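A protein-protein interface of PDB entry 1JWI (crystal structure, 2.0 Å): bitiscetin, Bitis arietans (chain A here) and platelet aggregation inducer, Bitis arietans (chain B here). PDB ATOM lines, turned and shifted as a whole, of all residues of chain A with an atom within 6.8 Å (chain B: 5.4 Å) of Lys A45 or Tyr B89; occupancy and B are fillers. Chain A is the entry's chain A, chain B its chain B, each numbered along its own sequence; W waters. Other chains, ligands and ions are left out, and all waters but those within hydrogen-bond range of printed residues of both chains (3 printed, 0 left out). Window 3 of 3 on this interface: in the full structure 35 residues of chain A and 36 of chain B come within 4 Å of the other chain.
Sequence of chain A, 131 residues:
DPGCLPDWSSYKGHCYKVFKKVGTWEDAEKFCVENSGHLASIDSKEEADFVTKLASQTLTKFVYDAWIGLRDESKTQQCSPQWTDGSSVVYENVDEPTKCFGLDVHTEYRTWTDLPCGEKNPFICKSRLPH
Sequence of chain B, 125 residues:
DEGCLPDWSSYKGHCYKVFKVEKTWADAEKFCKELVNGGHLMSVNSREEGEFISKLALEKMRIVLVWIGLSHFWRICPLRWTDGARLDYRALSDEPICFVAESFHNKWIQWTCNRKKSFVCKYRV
N of Trp A112 is in hydrogen-bond range of O of Ala B91.
The side-chain hydroxyl of Ser A44 sits at hydrogen-bond distance from the backbone NH of Glu A47 (3.1 Å).
OD1 of Asp A49 is in salt-bridge range of NZ of Lys A45 (2.9 Å).
The backbone NH of Asp A43 sits at hydrogen-bond distance from the side-chain carboxylate of Glu A47 (2.9 Å).
The backbone carbonyl oxygen (O) of Leu B87 sits at hydrogen-bond distance from the guanidinium group (NH1) of Arg B90.
Among the printed residues, pairs that only touch across the chains: Ile A42 with Trp B81 (3.5 Å), Ile A42 with Tyr B89 (3.9 Å), Asp A43 with Asp B88 (3.2 Å), Asp A43 with Tyr B89 (3.6 Å), Ser A44 with Tyr B89 (3.8 Å), Lys A45 with Tyr B89 (3.0 Å), Ala A48 with Tyr B89 (3.6 Å), Trp A112 with Trp B81 (3.6 Å), Trp A112 with Tyr B89 (3.5 Å) and Trp A112 with Arg B90 (3.5 Å).
Lys A45 touches one residue of chain B.
Glu A47 touches none of the printed residues of chain B.
Of the printed residues of chain B, Ala A48 touches Tyr B89.
Of the printed residues of chain B, Trp A112 touches Trp B81, Tyr B89, Arg B90 and Ala B91.
Tyr B89 touches six residues of chain A.
Hydrophobic or aromatic side chains of chain A that line the printed part of chain B: Ile A42, Ala A48 and Trp A112.
Among the printed residues, 11 pairs touch across the chains.
Water W1 lies within hydrogen-bond range of OH of Tyr B89 (2.6 Å) and O of Arg A110 (2.8 Å).
Water W2 bridges the side-chain carboxylate (OD1) of Asp A43 (2.6 Å) and the side-chain carboxylate (OD1) of Asp B88 (3.0 Å).
Water W3 lies within hydrogen-bond range of O of Tyr B89 (2.6 Å), O of Ile A42 (2.7 Å), N of Asp B88 (3.1 Å) and NE1 of Trp B81 (3.2 Å).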
ATOM      1  N   TYR A  11      19.731  22.175 -18.809  1.00  0.00           N
ATOM      2  CA  TYR A  11      18.530  23.000 -18.788  1.00  0.00           C
ATOM      3  C   TYR A  11      17.531  22.551 -17.723  1.00  0.00           C
ATOM      4  O   TYR A  11      17.095  21.400 -17.712  1.00  0.00           O
ATOM      5  CB  TYR A  11      17.858  22.994 -20.167  1.00  0.00           C
ATOM      6  CG  TYR A  11      16.571  23.785 -20.215  1.00  0.00           C
ATOM      7  CD1 TYR A  11      15.354  23.203 -19.848  1.00  0.00           C
ATOM      8  CD2 TYR A  11      16.571  25.131 -20.577  1.00  0.00           C
ATOM      9  CE1 TYR A  11      14.174  23.946 -19.834  1.00  0.00           C
ATOM     10  CE2 TYR A  11      15.394  25.884 -20.564  1.00  0.00           C
ATOM     11  CZ  TYR A  11      14.202  25.287 -20.191  1.00  0.00           C
ATOM     12  OH  TYR A  11      13.042  26.028 -20.152  1.00  0.00           O
ATOM     13  N   ILE A  42       8.880  16.640 -23.820  1.00  0.00           N
ATOM     14  CA  ILE A  42       8.770  18.095 -23.697  1.00  0.00           C
ATOM     15  C   ILE A  42       7.520  18.374 -22.868  1.00  0.00           C
ATOM     16  O   ILE A  42       6.431  17.949 -23.234  1.00  0.00           O
ATOM     17  CB  ILE A  42       8.670  18.740 -25.111  1.00  0.00           C
ATOM     18  CG1 ILE A  42       9.982  18.479 -25.870  1.00  0.00           C
ATOM     19  CG2 ILE A  42       8.394  20.229 -25.008  1.00  0.00           C
ATOM     20  CD1 ILE A  42       9.960  18.896 -27.322  1.00  0.00           C
ATOM     21  N   ASP A  43       7.671  19.078 -21.750  1.00  0.00           N
ATOM     22  CA  ASP A  43       6.515  19.310 -20.888  1.00  0.00           C
ATOM     23  C   ASP A  43       5.961  20.723 -20.848  1.00  0.00           C
ATOM     24  O   ASP A  43       4.911  20.950 -20.256  1.00  0.00           O
ATOM     25  CB  ASP A  43       6.835  18.835 -19.463  1.00  0.00           C
ATOM     26  CG  ASP A  43       5.604  18.311 -18.726  1.00  0.00           C
ATOM     27  OD1 ASP A  43       5.759  17.798 -17.594  1.00  0.00           O
ATOM     28  OD2 ASP A  43       4.482  18.402 -19.272  1.00  0.00           O
ATOM     29  N   SER A  44       6.648  21.666 -21.483  1.00  0.00           N
ATOM     30  CA  SER A  44       6.189  23.052 -21.496  1.00  0.00           C
ATOM     31  C   SER A  44       6.667  23.791 -22.742  1.00  0.00           C
ATOM     32  O   SER A  44       7.609  23.358 -23.412  1.00  0.00           O
ATOM     33  CB  SER A  44       6.696  23.791 -20.255  1.00  0.00           C
ATOM     34  OG  SER A  44       8.102  23.970 -20.321  1.00  0.00           O
ATOM     35  N   LYS A  45       6.020  24.912 -23.049  1.00  0.00           N
ATOM     36  CA  LYS A  45       6.406  25.702 -24.214  1.00  0.00           C
ATOM     37  C   LYS A  45       7.838  26.190 -24.047  1.00  0.00           C
ATOM     38  O   LYS A  45       8.587  26.261 -25.019  1.00  0.00           O
ATOM     39  CB  LYS A  45       5.475  26.903 -24.395  1.00  0.00           C
ATOM     40  CG  LYS A  45       5.819  27.800 -25.589  1.00  0.00           C
ATOM     41  CD  LYS A  45       5.760  27.032 -26.912  1.00  0.00           C
ATOM     42  CE  LYS A  45       5.662  27.972 -28.115  1.00  0.00           C
ATOM     43  NZ  LYS A  45       6.794  28.941 -28.177  1.00  0.00           N
ATOM     44  N   GLU A  46       8.220  26.523 -22.815  1.00  0.00           N
ATOM     45  CA  GLU A  46       9.572  26.998 -22.565  1.00  0.00           C
ATOM     46  C   GLU A  46      10.597  25.901 -22.835  1.00  0.00           C
ATOM     47  O   GLU A  46      11.636  26.155 -23.451  1.00  0.00           O
ATOM     48  CB  GLU A  46       9.708  27.517 -21.129  1.00  0.00           C
ATOM     49  CG  GLU A  46      10.778  28.602 -21.006  1.00  0.00           C
ATOM     50  CD  GLU A  46      10.653  29.417 -19.733  1.00  0.00           C
ATOM     51  OE1 GLU A  46      11.161  28.963 -18.687  1.00  0.00           O
ATOM     52  OE2 GLU A  46      10.033  30.507 -19.782  1.00  0.00           O
ATOM     53  N   GLU A  47      10.318  24.682 -22.380  1.00  0.00           N
ATOM     54  CA  GLU A  47      11.245  23.578 -22.634  1.00  0.00           C
ATOM     55  C   GLU A  47      11.282  23.340 -24.147  1.00  0.00           C
ATOM     56  O   GLU A  47      12.341  23.090 -24.723  1.00  0.00           O
ATOM     57  CB  GLU A  47      10.802  22.290 -21.925  1.00  0.00           C
ATOM     58  CG  GLU A  47      11.736  21.117 -22.211  1.00  0.00           C
ATOM     59  CD  GLU A  47      11.439  19.867 -21.395  1.00  0.00           C
ATOM     60  OE1 GLU A  47      12.332  18.998 -21.313  1.00  0.00           O
ATOM     61  OE2 GLU A  47      10.328  19.741 -20.845  1.00  0.00           O
ATOM     62  N   ALA A  48      10.116  23.430 -24.783  1.00  0.00           N
ATOM     63  CA  ALA A  48      10.005  23.236 -26.227  1.00  0.00           C
ATOM     64  C   ALA A  48      10.925  24.197 -26.976  1.00  0.00           C
ATOM     65  O   ALA A  48      11.655  23.791 -27.879  1.00  0.00           O
ATOM     66  CB  ALA A  48       8.553  23.443 -26.675  1.00  0.00           C
ATOM     67  N   ASP A  49      10.874  25.474 -26.602  1.00  0.00           N
ATOM     68  CA  ASP A  49      11.697  26.490 -27.248  1.00  0.00           C
ATOM     69  C   ASP A  49      13.182  26.194 -27.080  1.00  0.00           C
ATOM     70  O   ASP A  49      13.982  26.493 -27.965  1.00  0.00           O
ATOM     71  CB  ASP A  49      11.362  27.879 -26.695  1.00  0.00           C
ATOM     72  CG  ASP A  49      10.002  28.380 -27.161  1.00  0.00           C
ATOM     73  OD1 ASP A  49       9.450  27.813 -28.131  1.00  0.00           O
ATOM     74  OD2 ASP A  49       9.490  29.355 -26.572  1.00  0.00           O
ATOM     75  N   PHE A  50      13.548  25.596 -25.950  1.00  0.00           N
ATOM     76  CA  PHE A  50      14.944  25.254 -25.709  1.00  0.00           C
ATOM     77  C   PHE A  50      15.368  24.142 -26.660  1.00  0.00           C
ATOM     78  O   PHE A  50      16.393  24.250 -27.333  1.00  0.00           O
ATOM     79  CB  PHE A  50      15.158  24.786 -24.266  1.00  0.00           C
ATOM     80  CG  PHE A  50      16.514  24.170 -24.033  1.00  0.00           C
ATOM     81  CD1 PHE A  50      17.670  24.939 -24.124  1.00  0.00           C
ATOM     82  CD2 PHE A  50      16.637  22.805 -23.789  1.00  0.00           C
ATOM     83  CE1 PHE A  50      18.930  24.357 -23.977  1.00  0.00           C
ATOM     84  CE2 PHE A  50      17.891  22.211 -23.642  1.00  0.00           C
ATOM     85  CZ  PHE A  50      19.040  22.990 -23.739  1.00  0.00           C
ATOM     86  N   ARG A 110       9.934  23.675 -34.974  1.00  0.00           N
ATOM     87  CA  ARG A 110       9.022  24.372 -34.074  1.00  0.00           C
ATOM     88  C   ARG A 110       7.801  23.520 -33.708  1.00  0.00           C
ATOM     89  O   ARG A 110       7.226  23.681 -32.632  1.00  0.00           O
ATOM     90  CB  ARG A 110       8.552  25.682 -34.715  1.00  0.00           C
ATOM     91  CG  ARG A 110       7.726  26.559 -33.794  1.00  0.00           C
ATOM     92  CD  ARG A 110       8.540  27.014 -32.578  1.00  0.00           C
ATOM     93  NE  ARG A 110       9.723  27.794 -32.945  1.00  0.00           N
ATOM     94  CZ  ARG A 110      10.583  28.311 -32.069  1.00  0.00           C
ATOM     95  NH1 ARG A 110      10.399  28.134 -30.767  1.00  0.00           N
ATOM     96  NH2 ARG A 110      11.628  29.009 -32.495  1.00  0.00           N
ATOM     97  N   TRP A 112       5.573  19.446 -34.077  1.00  0.00           N
ATOM     98  CA  TRP A 112       5.771  18.000 -34.127  1.00  0.00           C
ATOM     99  C   TRP A 112       5.009  17.366 -35.290  1.00  0.00           C
ATOM    100  O   TRP A 112       3.912  17.804 -35.632  1.00  0.00           O
ATOM    101  CB  TRP A 112       5.335  17.361 -32.807  1.00  0.00           C
ATOM    102  CG  TRP A 112       5.979  17.981 -31.591  1.00  0.00           C
ATOM    103  CD1 TRP A 112       7.121  18.738 -31.558  1.00  0.00           C
ATOM    104  CD2 TRP A 112       5.545  17.853 -30.229  1.00  0.00           C
ATOM    105  NE1 TRP A 112       7.420  19.087 -30.259  1.00  0.00           N
ATOM    106  CE2 TRP A 112       6.470  18.559 -29.425  1.00  0.00           C
ATOM    107  CE3 TRP A 112       4.464  17.209 -29.611  1.00  0.00           C
ATOM    108  CZ2 TRP A 112       6.346  18.640 -28.032  1.00  0.00           C
ATOM    109  CZ3 TRP A 112       4.340  17.288 -28.219  1.00  0.00           C
ATOM    110  CH2 TRP A 112       5.278  18.000 -27.449  1.00  0.00           C
ATOM    111  N   TRP B  81       4.763   9.414 -23.782  1.00  0.00           N
ATOM    112  CA  TRP B  81       6.174   9.779 -23.764  1.00  0.00           C
ATOM    113  C   TRP B  81       6.924   8.533 -23.319  1.00  0.00           C
ATOM    114  O   TRP B  81       6.479   7.803 -22.430  1.00  0.00           O
ATOM    115  CB  TRP B  81       6.460  10.907 -22.775  1.00  0.00           C
ATOM    116  CG  TRP B  81       6.035  12.254 -23.244  1.00  0.00           C
ATOM    117  CD1 TRP B  81       5.101  13.060 -22.665  1.00  0.00           C
ATOM    118  CD2 TRP B  81       6.546  12.969 -24.376  1.00  0.00           C
ATOM    119  NE1 TRP B  81       4.997  14.238 -23.366  1.00  0.00           N
ATOM    120  CE2 TRP B  81       5.871  14.210 -24.422  1.00  0.00           C
ATOM    121  CE3 TRP B  81       7.505  12.684 -25.358  1.00  0.00           C
ATOM    122  CZ2 TRP B  81       6.126  15.172 -25.414  1.00  0.00           C
ATOM    123  CZ3 TRP B  81       7.761  13.638 -26.346  1.00  0.00           C
ATOM    124  CH2 TRP B  81       7.070  14.868 -26.363  1.00  0.00           C
ATOM    125  N   LEU B  87       1.374  13.784 -21.068  1.00  0.00           N
ATOM    126  CA  LEU B  87       1.319  14.635 -22.244  1.00  0.00           C
ATOM    127  C   LEU B  87       0.526  15.900 -21.928  1.00  0.00           C
ATOM    128  O   LEU B  87      -0.694  15.943 -22.084  1.00  0.00           O
ATOM    129  CB  LEU B  87       0.680  13.889 -23.424  1.00  0.00           C
ATOM    130  CG  LEU B  87       0.599  14.670 -24.745  1.00  0.00           C
ATOM    131  CD1 LEU B  87       1.995  15.096 -25.179  1.00  0.00           C
ATOM    132  CD2 LEU B  87      -0.053  13.814 -25.822  1.00  0.00           C
ATOM    133  N   ASP B  88       1.232  16.923 -21.463  1.00  0.00           N
ATOM    134  CA  ASP B  88       0.623  18.205 -21.130  1.00  0.00           C
ATOM    135  C   ASP B  88       0.720  19.096 -22.361  1.00  0.00           C
ATOM    136  O   ASP B  88      -0.248  19.272 -23.106  1.00  0.00           O
ATOM    137  CB  ASP B  88       1.372  18.855 -19.962  1.00  0.00           C
ATOM    138  CG  ASP B  88       0.522  18.964 -18.710  1.00  0.00           C
ATOM    139  OD1 ASP B  88       1.091  19.210 -17.619  1.00  0.00           O
ATOM    140  OD2 ASP B  88      -0.716  18.812 -18.819  1.00  0.00           O
ATOM    141  N   TYR B  89       1.904  19.654 -22.569  1.00  0.00           N
ATOM    142  CA  TYR B  89       2.152  20.516 -23.712  1.00  0.00           C
ATOM    143  C   TYR B  89       2.250  19.679 -24.990  1.00  0.00           C
ATOM    144  O   TYR B  89       2.832  18.594 -24.990  1.00  0.00           O
ATOM    145  CB  TYR B  89       3.458  21.287 -23.502  1.00  0.00           C
ATOM    146  CG  TYR B  89       3.872  22.117 -24.692  1.00  0.00           C
ATOM    147  CD1 TYR B  89       3.322  23.377 -24.918  1.00  0.00           C
ATOM    148  CD2 TYR B  89       4.794  21.624 -25.617  1.00  0.00           C
ATOM    149  CE1 TYR B  89       3.678  24.126 -26.037  1.00  0.00           C
ATOM    150  CE2 TYR B  89       5.153  22.365 -26.738  1.00  0.00           C
ATOM    151  CZ  TYR B  89       4.594  23.612 -26.942  1.00  0.00           C
ATOM    152  OH  TYR B  89       4.947  24.339 -28.054  1.00  0.00           O
ATOM    153  N   ARG B  90       1.675  20.184 -26.074  1.00  0.00           N
ATOM    154  CA  ARG B  90       1.730  19.481 -27.348  1.00  0.00           C
ATOM    155  C   ARG B  90       1.908  20.474 -28.477  1.00  0.00           C
ATOM    156  O   ARG B  90       1.351  21.567 -28.449  1.00  0.00           O
ATOM    157  CB  ARG B  90       0.454  18.662 -27.576  1.00  0.00           C
ATOM    158  CG  ARG B  90      -0.821  19.472 -27.588  1.00  0.00           C
ATOM    159  CD  ARG B  90      -1.794  18.926 -26.550  1.00  0.00           C
ATOM    160  NE  ARG B  90      -2.170  17.541 -26.819  1.00  0.00           N
ATOM    161  CZ  ARG B  90      -2.534  16.674 -25.878  1.00  0.00           C
ATOM    162  NH1 ARG B  90      -2.566  17.050 -24.604  1.00  0.00           N
ATOM    163  NH2 ARG B  90      -2.870  15.433 -26.210  1.00  0.00           N
ATOM    164  N   ALA B  91       2.705  20.092 -29.466  1.00  0.00           N
ATOM    165  CA  ALA B  91       2.944  20.945 -30.614  1.00  0.00           C
ATOM    166  C   ALA B  91       2.509  20.187 -31.858  1.00  0.00           C
ATOM    167  O   ALA B  91       3.173  20.220 -32.892  1.00  0.00           O
ATOM    168  CB  ALA B  91       4.419  21.316 -30.699  1.00  0.00           C
HETATM  169  O   HOH W   1       6.726  24.063 -29.891  1.00  0.00           O
HETATM  170  O   HOH W   2       3.410  17.679 -16.552  1.00  0.00           O
HETATM  171  O   HOH W   3       3.882  17.252 -22.965  1.00  0.00           O
